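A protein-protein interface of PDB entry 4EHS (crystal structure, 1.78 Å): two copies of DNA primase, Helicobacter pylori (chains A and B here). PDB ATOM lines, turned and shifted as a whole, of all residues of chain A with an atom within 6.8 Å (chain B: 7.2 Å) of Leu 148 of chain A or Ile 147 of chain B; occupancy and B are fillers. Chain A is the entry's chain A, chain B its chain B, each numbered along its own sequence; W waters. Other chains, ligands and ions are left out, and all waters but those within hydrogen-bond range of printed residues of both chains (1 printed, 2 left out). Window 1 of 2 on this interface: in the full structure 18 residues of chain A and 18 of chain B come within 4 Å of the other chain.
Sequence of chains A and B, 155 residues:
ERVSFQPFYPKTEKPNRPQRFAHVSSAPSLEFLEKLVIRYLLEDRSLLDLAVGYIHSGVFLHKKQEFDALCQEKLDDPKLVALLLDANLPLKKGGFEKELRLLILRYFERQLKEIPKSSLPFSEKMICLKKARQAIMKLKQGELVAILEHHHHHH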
ATOM      1  N   GLY A  53     -13.987 -15.536   9.251  1.00  0.00           N
ATOM      2  CA  GLY A  53     -14.972 -15.780   8.172  1.00  0.00           C
ATOM      3  C   GLY A  53     -16.411 -15.482   8.579  1.00  0.00           C
ATOM      4  O   GLY A  53     -17.272 -15.272   7.703  1.00  0.00           O
ATOM      5  N   TYR A  54     -16.677 -15.437   9.902  1.00  0.00           N
ATOM      6  CA  TYR A  54     -18.103 -15.477  10.396  1.00  0.00           C
ATOM      7  C   TYR A  54     -18.379 -14.395  11.443  1.00  0.00           C
ATOM      8  O   TYR A  54     -19.519 -13.915  11.561  1.00  0.00           O
ATOM      9  CB  TYR A  54     -18.420 -16.846  10.998  1.00  0.00           C
ATOM     10  CG  TYR A  54     -18.269 -17.941   9.979  1.00  0.00           C
ATOM     11  CD1 TYR A  54     -19.235 -18.150   8.991  1.00  0.00           C
ATOM     12  CD2 TYR A  54     -17.098 -18.714   9.946  1.00  0.00           C
ATOM     13  CE1 TYR A  54     -19.066 -19.171   8.029  1.00  0.00           C
ATOM     14  CE2 TYR A  54     -16.905 -19.694   8.981  1.00  0.00           C
ATOM     15  CZ  TYR A  54     -17.898 -19.881   8.011  1.00  0.00           C
ATOM     16  OH  TYR A  54     -17.707 -20.868   7.073  1.00  0.00           O
ATOM     17  N   HIS A  56     -17.030 -10.828  13.742  1.00  0.00           N
ATOM     18  CA  HIS A  56     -16.148  -9.688  13.928  1.00  0.00           C
ATOM     19  C   HIS A  56     -16.314  -9.158  15.331  1.00  0.00           C
ATOM     20  O   HIS A  56     -17.184  -9.608  16.132  1.00  0.00           O
ATOM     21  CB  HIS A  56     -16.471  -8.613  12.858  1.00  0.00           C
ATOM     22  CG  HIS A  56     -17.911  -8.154  12.913  1.00  0.00           C
ATOM     23  ND1 HIS A  56     -18.347  -7.284  13.836  1.00  0.00           N
ATOM     24  CD2 HIS A  56     -19.024  -8.534  12.183  1.00  0.00           C
ATOM     25  CE1 HIS A  56     -19.678  -7.095  13.707  1.00  0.00           C
ATOM     26  NE2 HIS A  56     -20.095  -7.862  12.705  1.00  0.00           N
ATOM     27  N   TYR A 107     -26.465 -14.334  18.699  1.00  0.00           N
ATOM     28  CA  TYR A 107     -26.519 -13.046  18.001  1.00  0.00           C
ATOM     29  C   TYR A 107     -27.820 -12.950  17.162  1.00  0.00           C
ATOM     30  O   TYR A 107     -28.531 -11.955  17.225  1.00  0.00           O
ATOM     31  CB  TYR A 107     -25.291 -12.924  17.088  1.00  0.00           C
ATOM     32  CG  TYR A 107     -25.361 -11.709  16.210  1.00  0.00           C
ATOM     33  CD1 TYR A 107     -24.867 -10.474  16.648  1.00  0.00           C
ATOM     34  CD2 TYR A 107     -25.920 -11.803  14.948  1.00  0.00           C
ATOM     35  CE1 TYR A 107     -24.950  -9.334  15.849  1.00  0.00           C
ATOM     36  CE2 TYR A 107     -26.024 -10.670  14.154  1.00  0.00           C
ATOM     37  CZ  TYR A 107     -25.509  -9.461  14.588  1.00  0.00           C
ATOM     38  OH  TYR A 107     -25.625  -8.348  13.736  1.00  0.00           O
ATOM     39  N   PHE A 108     -28.115 -13.952  16.386  1.00  0.00           N
ATOM     40  CA  PHE A 108     -29.321 -13.896  15.523  1.00  0.00           C
ATOM     41  C   PHE A 108     -30.630 -13.994  16.318  1.00  0.00           C
ATOM     42  O   PHE A 108     -31.639 -13.356  15.933  1.00  0.00           O
ATOM     43  CB  PHE A 108     -29.283 -14.922  14.409  1.00  0.00           C
ATOM     44  CG  PHE A 108     -28.342 -14.561  13.293  1.00  0.00           C
ATOM     45  CD1 PHE A 108     -28.646 -13.518  12.411  1.00  0.00           C
ATOM     46  CD2 PHE A 108     -27.167 -15.255  13.109  1.00  0.00           C
ATOM     47  CE1 PHE A 108     -27.762 -13.179  11.380  1.00  0.00           C
ATOM     48  CE2 PHE A 108     -26.301 -14.958  12.041  1.00  0.00           C
ATOM     49  CZ  PHE A 108     -26.567 -13.900  11.200  1.00  0.00           C
ATOM     50  N   LYS A 131     -33.606 -13.046   7.088  1.00  0.00           N
ATOM     51  CA  LYS A 131     -32.218 -13.485   7.160  1.00  0.00           C
ATOM     52  C   LYS A 131     -31.862 -14.050   8.526  1.00  0.00           C
ATOM     53  O   LYS A 131     -31.205 -15.104   8.610  1.00  0.00           O
ATOM     54  CB  LYS A 131     -31.295 -12.343   6.819  1.00  0.00           C
ATOM     55  CG  LYS A 131     -29.827 -12.807   6.723  1.00  0.00           C
ATOM     56  CD  LYS A 131     -28.889 -12.032   7.681  1.00  0.00           C
ATOM     57  CE  LYS A 131     -27.377 -12.253   7.404  1.00  0.00           C
ATOM     58  NZ  LYS A 131     -26.694 -11.040   6.871  1.00  0.00           N
ATOM     59  N   ALA A 146     -22.276 -16.482   8.518  1.00  0.00           N
ATOM     60  CA  ALA A 146     -21.589 -15.208   8.779  1.00  0.00           C
ATOM     61  C   ALA A 146     -22.513 -14.130   9.295  1.00  0.00           C
ATOM     62  O   ALA A 146     -23.663 -14.022   8.836  1.00  0.00           O
ATOM     63  CB  ALA A 146     -20.940 -14.740   7.470  1.00  0.00           C
ATOM     64  N   ILE A 147     -22.041 -13.314  10.233  1.00  0.00           N
ATOM     65  CA  ILE A 147     -22.696 -12.052  10.618  1.00  0.00           C
ATOM     66  C   ILE A 147     -22.117 -10.848   9.846  1.00  0.00           C
ATOM     67  O   ILE A 147     -21.029 -10.313  10.214  1.00  0.00           O
ATOM     68  CB  ILE A 147     -22.433 -11.782  12.127  1.00  0.00           C
ATOM     69  CG1 ILE A 147     -22.943 -12.981  12.891  1.00  0.00           C
ATOM     70  CG2 ILE A 147     -22.980 -10.411  12.584  1.00  0.00           C
ATOM     71  CD1 ILE A 147     -22.531 -13.027  14.361  1.00  0.00           C
ATOM     72  N   LEU A 148     -22.804 -10.356   8.828  1.00  0.00           N
ATOM     73  CA  LEU A 148     -22.225  -9.204   8.056  1.00  0.00           C
ATOM     74  C   LEU A 148     -22.289  -7.870   8.803  1.00  0.00           C
ATOM     75  O   LEU A 148     -21.265  -7.194   8.967  1.00  0.00           O
ATOM     76  CB  LEU A 148     -22.917  -9.048   6.689  1.00  0.00           C
ATOM     77  CG  LEU A 148     -22.461  -9.907   5.533  1.00  0.00           C
ATOM     78  CD1 LEU A 148     -22.435 -11.387   5.912  1.00  0.00           C
ATOM     79  CD2 LEU A 148     -23.382  -9.646   4.342  1.00  0.00           C
ATOM     80  N   GLU A 149     -23.507  -7.526   9.236  1.00  0.00           N
ATOM     81  CA  GLU A 149     -23.938  -6.198   9.707  1.00  0.00           C
ATOM     82  C   GLU A 149     -23.673  -5.896  11.191  1.00  0.00           C
ATOM     83  O   GLU A 149     -22.580  -6.158  11.720  1.00  0.00           O
ATOM     84  CB  GLU A 149     -25.435  -5.983   9.329  1.00  0.00           C
ATOM     85  CG  GLU A 149     -26.507  -6.924   9.901  1.00  0.00           C
ATOM     86  CD  GLU A 149     -26.080  -8.399  10.145  1.00  0.00           C
ATOM     87  OE1 GLU A 149     -25.639  -9.142   9.218  1.00  0.00           O
ATOM     88  OE2 GLU A 149     -26.214  -8.833  11.307  1.00  0.00           O
ATOM     89  N   ALA B  51     -28.546 -12.899  -1.603  1.00  0.00           N
ATOM     90  CA  ALA B  51     -27.404 -11.900  -1.648  1.00  0.00           C
ATOM     91  C   ALA B  51     -27.021 -11.291  -0.291  1.00  0.00           C
ATOM     92  O   ALA B  51     -25.828 -11.136  -0.004  1.00  0.00           O
ATOM     93  CB  ALA B  51     -27.707 -10.750  -2.605  1.00  0.00           C
ATOM     94  N   VAL B  52     -28.017 -10.956   0.524  1.00  0.00           N
ATOM     95  CA  VAL B  52     -27.732 -10.256   1.762  1.00  0.00           C
ATOM     96  C   VAL B  52     -27.051 -11.177   2.785  1.00  0.00           C
ATOM     97  O   VAL B  52     -26.650 -10.680   3.803  1.00  0.00           O
ATOM     98  CB  VAL B  52     -28.966  -9.591   2.320  1.00  0.00           C
ATOM     99  CG1 VAL B  52     -29.484  -8.581   1.276  1.00  0.00           C
ATOM    100  CG2 VAL B  52     -30.008 -10.673   2.749  1.00  0.00           C
ATOM    101  N   GLY B  53     -26.969 -12.479   2.509  1.00  0.00           N
ATOM    102  CA  GLY B  53     -26.119 -13.389   3.304  1.00  0.00           C
ATOM    103  C   GLY B  53     -24.629 -13.102   3.078  1.00  0.00           C
ATOM    104  O   GLY B  53     -23.757 -13.537   3.848  1.00  0.00           O
ATOM    105  N   TYR B  54     -24.332 -12.424   1.983  1.00  0.00           N
ATOM    106  CA  TYR B  54     -22.912 -12.307   1.534  1.00  0.00           C
ATOM    107  C   TYR B  54     -22.411 -10.912   1.285  1.00  0.00           C
ATOM    108  O   TYR B  54     -21.211 -10.667   1.441  1.00  0.00           O
ATOM    109  CB  TYR B  54     -22.655 -13.144   0.269  1.00  0.00           C
ATOM    110  CG  TYR B  54     -23.032 -14.587   0.486  1.00  0.00           C
ATOM    111  CD1 TYR B  54     -22.208 -15.431   1.233  1.00  0.00           C
ATOM    112  CD2 TYR B  54     -24.269 -15.063   0.062  1.00  0.00           C
ATOM    113  CE1 TYR B  54     -22.583 -16.744   1.482  1.00  0.00           C
ATOM    114  CE2 TYR B  54     -24.645 -16.391   0.299  1.00  0.00           C
ATOM    115  CZ  TYR B  54     -23.814 -17.206   1.039  1.00  0.00           C
ATOM    116  OH  TYR B  54     -24.198 -18.502   1.271  1.00  0.00           O
ATOM    117  N   ILE B  55     -23.271 -10.035   0.794  1.00  0.00           N
ATOM    118  CA  ILE B  55     -22.827  -8.688   0.387  1.00  0.00           C
ATOM    119  C   ILE B  55     -23.678  -7.635   1.112  1.00  0.00           C
ATOM    120  O   ILE B  55     -24.756  -7.950   1.630  1.00  0.00           O
ATOM    121  CB  ILE B  55     -22.881  -8.428  -1.138  1.00  0.00           C
ATOM    122  CG1 ILE B  55     -24.291  -8.581  -1.709  1.00  0.00           C
ATOM    123  CG2 ILE B  55     -21.940  -9.386  -1.890  1.00  0.00           C
ATOM    124  CD1 ILE B  55     -24.404  -8.109  -3.167  1.00  0.00           C
ATOM    125  N   HIS B  56     -23.207  -6.401   1.084  1.00  0.00           N
ATOM    126  CA  HIS B  56     -23.872  -5.227   1.732  1.00  0.00           C
ATOM    127  C   HIS B  56     -23.538  -4.033   0.861  1.00  0.00           C
ATOM    128  O   HIS B  56     -22.757  -4.183  -0.098  1.00  0.00           O
ATOM    129  CB  HIS B  56     -23.426  -5.052   3.211  1.00  0.00           C
ATOM    130  CG  HIS B  56     -21.946  -4.983   3.408  1.00  0.00           C
ATOM    131  ND1 HIS B  56     -21.223  -3.900   3.099  1.00  0.00           N
ATOM    132  CD2 HIS B  56     -21.039  -5.952   3.831  1.00  0.00           C
ATOM    133  CE1 HIS B  56     -19.911  -4.151   3.309  1.00  0.00           C
ATOM    134  NE2 HIS B  56     -19.809  -5.415   3.763  1.00  0.00           N
ATOM    135  N   GLY B  58     -21.742  -1.607   1.088  1.00  0.00           N
ATOM    136  CA  GLY B  58     -20.340  -1.206   1.092  1.00  0.00           C
ATOM    137  C   GLY B  58     -19.507  -1.911   0.036  1.00  0.00           C
ATOM    138  O   GLY B  58     -18.470  -1.385  -0.373  1.00  0.00           O
ATOM    139  N   VAL B  59     -19.970  -3.072  -0.436  1.00  0.00           N
ATOM    140  CA  VAL B  59     -19.370  -3.811  -1.550  1.00  0.00           C
ATOM    141  C   VAL B  59     -19.380  -3.015  -2.874  1.00  0.00           C
ATOM    142  O   VAL B  59     -18.460  -3.172  -3.719  1.00  0.00           O
ATOM    143  CB  VAL B  59     -20.044  -5.213  -1.713  1.00  0.00           C
ATOM    144  CG1 VAL B  59     -19.370  -6.061  -2.754  1.00  0.00           C
ATOM    145  CG2 VAL B  59     -19.962  -5.948  -0.353  1.00  0.00           C
ATOM    146  N   LEU B 100     -22.960 -12.998  -8.842  1.00  0.00           N
ATOM    147  CA  LEU B 100     -22.674 -12.681  -7.411  1.00  0.00           C
ATOM    148  C   LEU B 100     -21.285 -13.162  -6.975  1.00  0.00           C
ATOM    149  O   LEU B 100     -20.530 -12.429  -6.314  1.00  0.00           O
ATOM    150  CB  LEU B 100     -23.739 -13.290  -6.475  1.00  0.00           C
ATOM    151  CG  LEU B 100     -23.554 -12.987  -4.974  1.00  0.00           C
ATOM    152  CD1 LEU B 100     -23.718 -11.521  -4.629  1.00  0.00           C
ATOM    153  CD2 LEU B 100     -24.604 -13.785  -4.228  1.00  0.00           C
ATOM    154  N   LEU B 103     -18.688 -10.946  -8.333  1.00  0.00           N
ATOM    155  CA  LEU B 103     -18.651  -9.631  -7.692  1.00  0.00           C
ATOM    156  C   LEU B 103     -17.868  -9.789  -6.357  1.00  0.00           C
ATOM    157  O   LEU B 103     -17.031  -8.939  -6.006  1.00  0.00           O
ATOM    158  CB  LEU B 103     -20.109  -9.078  -7.503  1.00  0.00           C
ATOM    159  CG  LEU B 103     -20.143  -7.754  -6.792  1.00  0.00           C
ATOM    160  CD1 LEU B 103     -19.719  -6.675  -7.802  1.00  0.00           C
ATOM    161  CD2 LEU B 103     -21.553  -7.446  -6.180  1.00  0.00           C
ATOM    162  N   ILE B 104     -18.110 -10.894  -5.633  1.00  0.00           N
ATOM    163  CA  ILE B 104     -17.365 -11.141  -4.373  1.00  0.00           C
ATOM    164  C   ILE B 104     -15.892 -11.372  -4.649  1.00  0.00           C
ATOM    165  O   ILE B 104     -15.044 -10.806  -3.954  1.00  0.00           O
ATOM    166  CB  ILE B 104     -18.000 -12.279  -3.581  1.00  0.00           C
ATOM    167  CG1 ILE B 104     -19.464 -11.901  -3.292  1.00  0.00           C
ATOM    168  CG2 ILE B 104     -17.216 -12.505  -2.280  1.00  0.00           C
ATOM    169  CD1 ILE B 104     -20.335 -13.050  -2.751  1.00  0.00           C
ATOM    170  N   LEU B 105     -15.574 -12.177  -5.686  1.00  0.00           N
ATOM    171  CA  LEU B 105     -14.179 -12.447  -6.063  1.00  0.00           C
ATOM    172  C   LEU B 105     -13.468 -11.140  -6.336  1.00  0.00           C
ATOM    173  O   LEU B 105     -12.340 -10.931  -5.864  1.00  0.00           O
ATOM    174  CB  LEU B 105     -14.089 -13.420  -7.283  1.00  0.00           C
ATOM    175  CG  LEU B 105     -12.699 -13.721  -7.891  1.00  0.00           C
ATOM    176  CD1 LEU B 105     -11.826 -14.281  -6.761  1.00  0.00           C
ATOM    177  CD2 LEU B 105     -12.861 -14.774  -8.988  1.00  0.00           C
ATOM    178  N   TYR B 107     -14.128  -8.158  -5.199  1.00  0.00           N
ATOM    179  CA  TYR B 107     -13.964  -7.437  -3.946  1.00  0.00           C
ATOM    180  C   TYR B 107     -12.697  -7.956  -3.233  1.00  0.00           C
ATOM    181  O   TYR B 107     -11.880  -7.163  -2.761  1.00  0.00           O
ATOM    182  CB  TYR B 107     -15.211  -7.675  -3.083  1.00  0.00           C
ATOM    183  CG  TYR B 107     -15.022  -7.179  -1.668  1.00  0.00           C
ATOM    184  CD1 TYR B 107     -15.380  -5.869  -1.335  1.00  0.00           C
ATOM    185  CD2 TYR B 107     -14.467  -7.983  -0.712  1.00  0.00           C
ATOM    186  CE1 TYR B 107     -15.232  -5.387  -0.058  1.00  0.00           C
ATOM    187  CE2 TYR B 107     -14.301  -7.511   0.561  1.00  0.00           C
ATOM    188  CZ  TYR B 107     -14.689  -6.237   0.881  1.00  0.00           C
ATOM    189  OH  TYR B 107     -14.471  -5.817   2.185  1.00  0.00           O
ATOM    190  N   PHE B 108     -12.558  -9.277  -3.132  1.00  0.00           N
ATOM    191  CA  PHE B 108     -11.383  -9.832  -2.419  1.00  0.00           C
ATOM    192  C   PHE B 108     -10.066  -9.664  -3.200  1.00  0.00           C
ATOM    193  O   PHE B 108      -9.028  -9.412  -2.588  1.00  0.00           O
ATOM    194  CB  PHE B 108     -11.608 -11.291  -2.055  1.00  0.00           C
ATOM    195  CG  PHE B 108     -12.518 -11.478  -0.884  1.00  0.00           C
ATOM    196  CD1 PHE B 108     -12.109 -11.091   0.412  1.00  0.00           C
ATOM    197  CD2 PHE B 108     -13.833 -12.029  -1.071  1.00  0.00           C
ATOM    198  CE1 PHE B 108     -12.960 -11.288   1.519  1.00  0.00           C
ATOM    199  CE2 PHE B 108     -14.659 -12.210   0.050  1.00  0.00           C
ATOM    200  CZ  PHE B 108     -14.238 -11.822   1.336  1.00  0.00           C
ATOM    201  N   ARG B 110      -9.470  -6.995  -4.961  1.00  0.00           N
ATOM    202  CA  ARG B 110      -9.135  -5.610  -4.624  1.00  0.00           C
ATOM    203  C   ARG B 110      -8.552  -5.531  -3.220  1.00  0.00           C
ATOM    204  O   ARG B 110      -7.637  -4.765  -3.008  1.00  0.00           O
ATOM    205  CB  ARG B 110     -10.338  -4.672  -4.726  1.00  0.00           C
ATOM    206  CG  ARG B 110     -10.771  -4.337  -6.156  1.00  0.00           C
ATOM    207  CD  ARG B 110     -11.753  -3.154  -6.213  1.00  0.00           C
ATOM    208  NE  ARG B 110     -12.873  -3.254  -5.249  1.00  0.00           N
ATOM    209  CZ  ARG B 110     -13.981  -3.965  -5.494  1.00  0.00           C
ATOM    210  NH1 ARG B 110     -14.097  -4.676  -6.629  1.00  0.00           N
ATOM    211  NH2 ARG B 110     -14.975  -4.007  -4.566  1.00  0.00           N
ATOM    212  N   GLN B 111      -9.027  -6.348  -2.262  1.00  0.00           N
ATOM    213  CA  GLN B 111      -8.464  -6.262  -0.918  1.00  0.00           C
ATOM    214  C   GLN B 111      -6.959  -6.621  -0.970  1.00  0.00           C
ATOM    215  O   GLN B 111      -6.151  -5.997  -0.264  1.00  0.00           O
ATOM    216  CB  GLN B 111      -9.111  -7.319   0.015  1.00  0.00           C
ATOM    217  CG  GLN B 111     -10.560  -7.086   0.339  1.00  0.00           C
ATOM    218  CD  GLN B 111     -10.707  -6.084   1.413  1.00  0.00           C
ATOM    219  OE1 GLN B 111     -10.864  -4.901   1.117  1.00  0.00           O
ATOM    220  NE2 GLN B 111     -10.658  -6.531   2.684  1.00  0.00           N
ATOM    221  N   LYS B 131      -7.391 -13.767   5.134  1.00  0.00           N
ATOM    222  CA  LYS B 131      -8.853 -13.914   4.967  1.00  0.00           C
ATOM    223  C   LYS B 131      -9.152 -13.785   3.467  1.00  0.00           C
ATOM    224  O   LYS B 131      -9.909 -14.597   2.890  1.00  0.00           O
ATOM    225  CB  LYS B 131      -9.510 -12.800   5.776  1.00  0.00           C
ATOM    226  CG  LYS B 131     -11.023 -12.772   5.945  1.00  0.00           C
ATOM    227  CD  LYS B 131     -11.432 -11.633   6.932  1.00  0.00           C
ATOM    228  CE  LYS B 131     -12.962 -11.384   6.967  1.00  0.00           C
ATOM    229  NZ  LYS B 131     -13.517 -10.836   5.670  1.00  0.00           N
ATOM    230  N   VAL B 145     -18.705 -16.596  -0.383  1.00  0.00           N
ATOM    231  CA  VAL B 145     -18.073 -16.252   0.887  1.00  0.00           C
ATOM    232  C   VAL B 145     -18.645 -14.914   1.292  1.00  0.00           C
ATOM    233  O   VAL B 145     -18.843 -14.034   0.446  1.00  0.00           O
ATOM    234  CB  VAL B 145     -16.496 -16.161   0.767  1.00  0.00           C
ATOM    235  CG1 VAL B 145     -15.907 -15.550   2.044  1.00  0.00           C
ATOM    236  CG2 VAL B 145     -15.857 -17.450   0.308  1.00  0.00           C
ATOM    237  N   ALA B 146     -19.009 -14.757   2.564  1.00  0.00           N
ATOM    238  CA  ALA B 146     -19.459 -13.459   3.077  1.00  0.00           C
ATOM    239  C   ALA B 146     -18.413 -12.382   3.173  1.00  0.00           C
ATOM    240  O   ALA B 146     -17.250 -12.652   3.560  1.00  0.00           O
ATOM    241  CB  ALA B 146     -20.101 -13.610   4.482  1.00  0.00           C
ATOM    242  N   ILE B 147     -18.795 -11.189   2.765  1.00  0.00           N
ATOM    243  CA  ILE B 147     -17.954 -10.012   2.985  1.00  0.00           C
ATOM    244  C   ILE B 147     -18.362  -9.404   4.307  1.00  0.00           C
ATOM    245  O   ILE B 147     -19.419  -8.704   4.403  1.00  0.00           O
ATOM    246  CB  ILE B 147     -18.083  -9.000   1.884  1.00  0.00           C
ATOM    247  CG1 ILE B 147     -17.634  -9.709   0.585  1.00  0.00           C
ATOM    248  CG2 ILE B 147     -17.272  -7.787   2.225  1.00  0.00           C
ATOM    249  CD1 ILE B 147     -18.008  -8.922  -0.659  1.00  0.00           C
ATOM    250  N   LEU B 148     -17.499  -9.666   5.298  1.00  0.00           N
ATOM    251  CA  LEU B 148     -17.587  -9.112   6.650  1.00  0.00           C
ATOM    252  C   LEU B 148     -16.374  -8.198   6.734  1.00  0.00           C
ATOM    253  O   LEU B 148     -16.519  -7.001   6.704  1.00  0.00           O
ATOM    254  CB  LEU B 148     -17.279 -10.192   7.668  1.00  0.00           C
ATOM    255  CG  LEU B 148     -18.212 -11.283   8.104  1.00  0.00           C
ATOM    256  CD1 LEU B 148     -18.145 -12.542   7.287  1.00  0.00           C
ATOM    257  CD2 LEU B 148     -17.634 -11.554   9.470  1.00  0.00           C
HETATM  258  O   HOH W   1     -16.429 -14.991   5.226  1.00  0.00           O
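Water W1 lies within hydrogen-bond range of O of Gly 53 of chain A (2.6 Å) and O of Ala 146 of chain B (3.0 Å).
Tyr 54 of chain A touches Leu 148 of chain B, and with the chains exchanged Leu 148 of chain A touches Tyr 54 of chain B.
Ala 146 of chain A touches its own counterpart, Ala 146 of chain B.
Ala 146 of chain A touches Leu 148 of chain B, and with the chains exchanged Leu 148 of chain A touches Ala 146 of chain B.
Ile 147 of chain A touches Leu 148 of chain B, and with the chains exchanged Leu 148 of chain A touches Ile 147 of chain B.
Positions printed for both chains: 53, 54, 56, 107, 108, 131, 146, 147 and 148.
The backbone carbonyl oxygen of Tyr 54 of chain A sits at hydrogen-bond distance from the backbone NH of Ile 147 of chain A (2.9 Å).
The side-chain amino group (NZ) of Lys 131 of chain A is in salt-bridge range of the side-chain carboxylate (OE1) of Glu 149 of chain A (3.2 Å).
The backbone carbonyl oxygen of Tyr 54 of chain B is in hydrogen-bond range of the backbone NH of Ile 147 of chain B, 2.8 Å away.
A ring nitrogen (NE2) of His 56 of chain B lies close to the backbone carbonyl oxygen (O) of Ile 147 of chain B (3.4 Å).
The backbone carbonyl oxygen (O) of Val 52 of chain B lies within hydrogen-bond range of the side-chain amino group (NZ) of Lys 131 of chain A, at 3.1 Å.
O of Gly 53 of chain A touches CD1 of Leu 148 of chain B, 2.9 Å away.
Tyr 54 of chain A touches Leu 148 of chain B.
CB of Ala 146 of chain A touches CB of Ala 146 of chain B, at 3.3 Å.
Ala 146 of chain A touches Leu 148 of chain B (CB to CD1, 3.6 Å).
Leu 148 of chain B touches Ile 147 of chain A (CG to O, 3.7 Å).
Leu 148 of chain A touches Val 52 of chain B.
C of Tyr 54 of chain B touches CD2 of Leu 148 of chain A, 3.4 Å away.
Leu 148 of chain A touches Ile 55 of chain B.
Leu 148 of chain A touches Ala 146 of chain B (CD1 to CB, 3.5 Å).
CG of Leu 148 of chain A touches O of Ile 147 of chain B (3.5 Å).
Of the 10 printed residues of chain A, 6 touch a printed residue of chain B.
Printed residues of chain A that touch a printed residue of chain B: Gly 53, Tyr 54, Lys 131, Ala 146, Ile 147 and Leu 148.
Among the printed residues, no Asp or Glu carboxylate lies within 4 Å of a Lys or Arg side-chain nitrogen of the other chain.
Leu 148 of chain A touches six residues of chain B.
Of the printed residues of chain A, Val 52 of chain B touches Lys 131 (3.1 Å) and Leu 148 (3.5 Å).
Of the printed residues of chain A, Ala 146 of chain B touches Ala 146 and Leu 148.
Of the printed residues of chain A, Ile 147 of chain B touches Leu 148.
The nearest printed residue of chain A that does not touch Val 52 of chain B is Glu 149 of chain A (5.7 Å).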
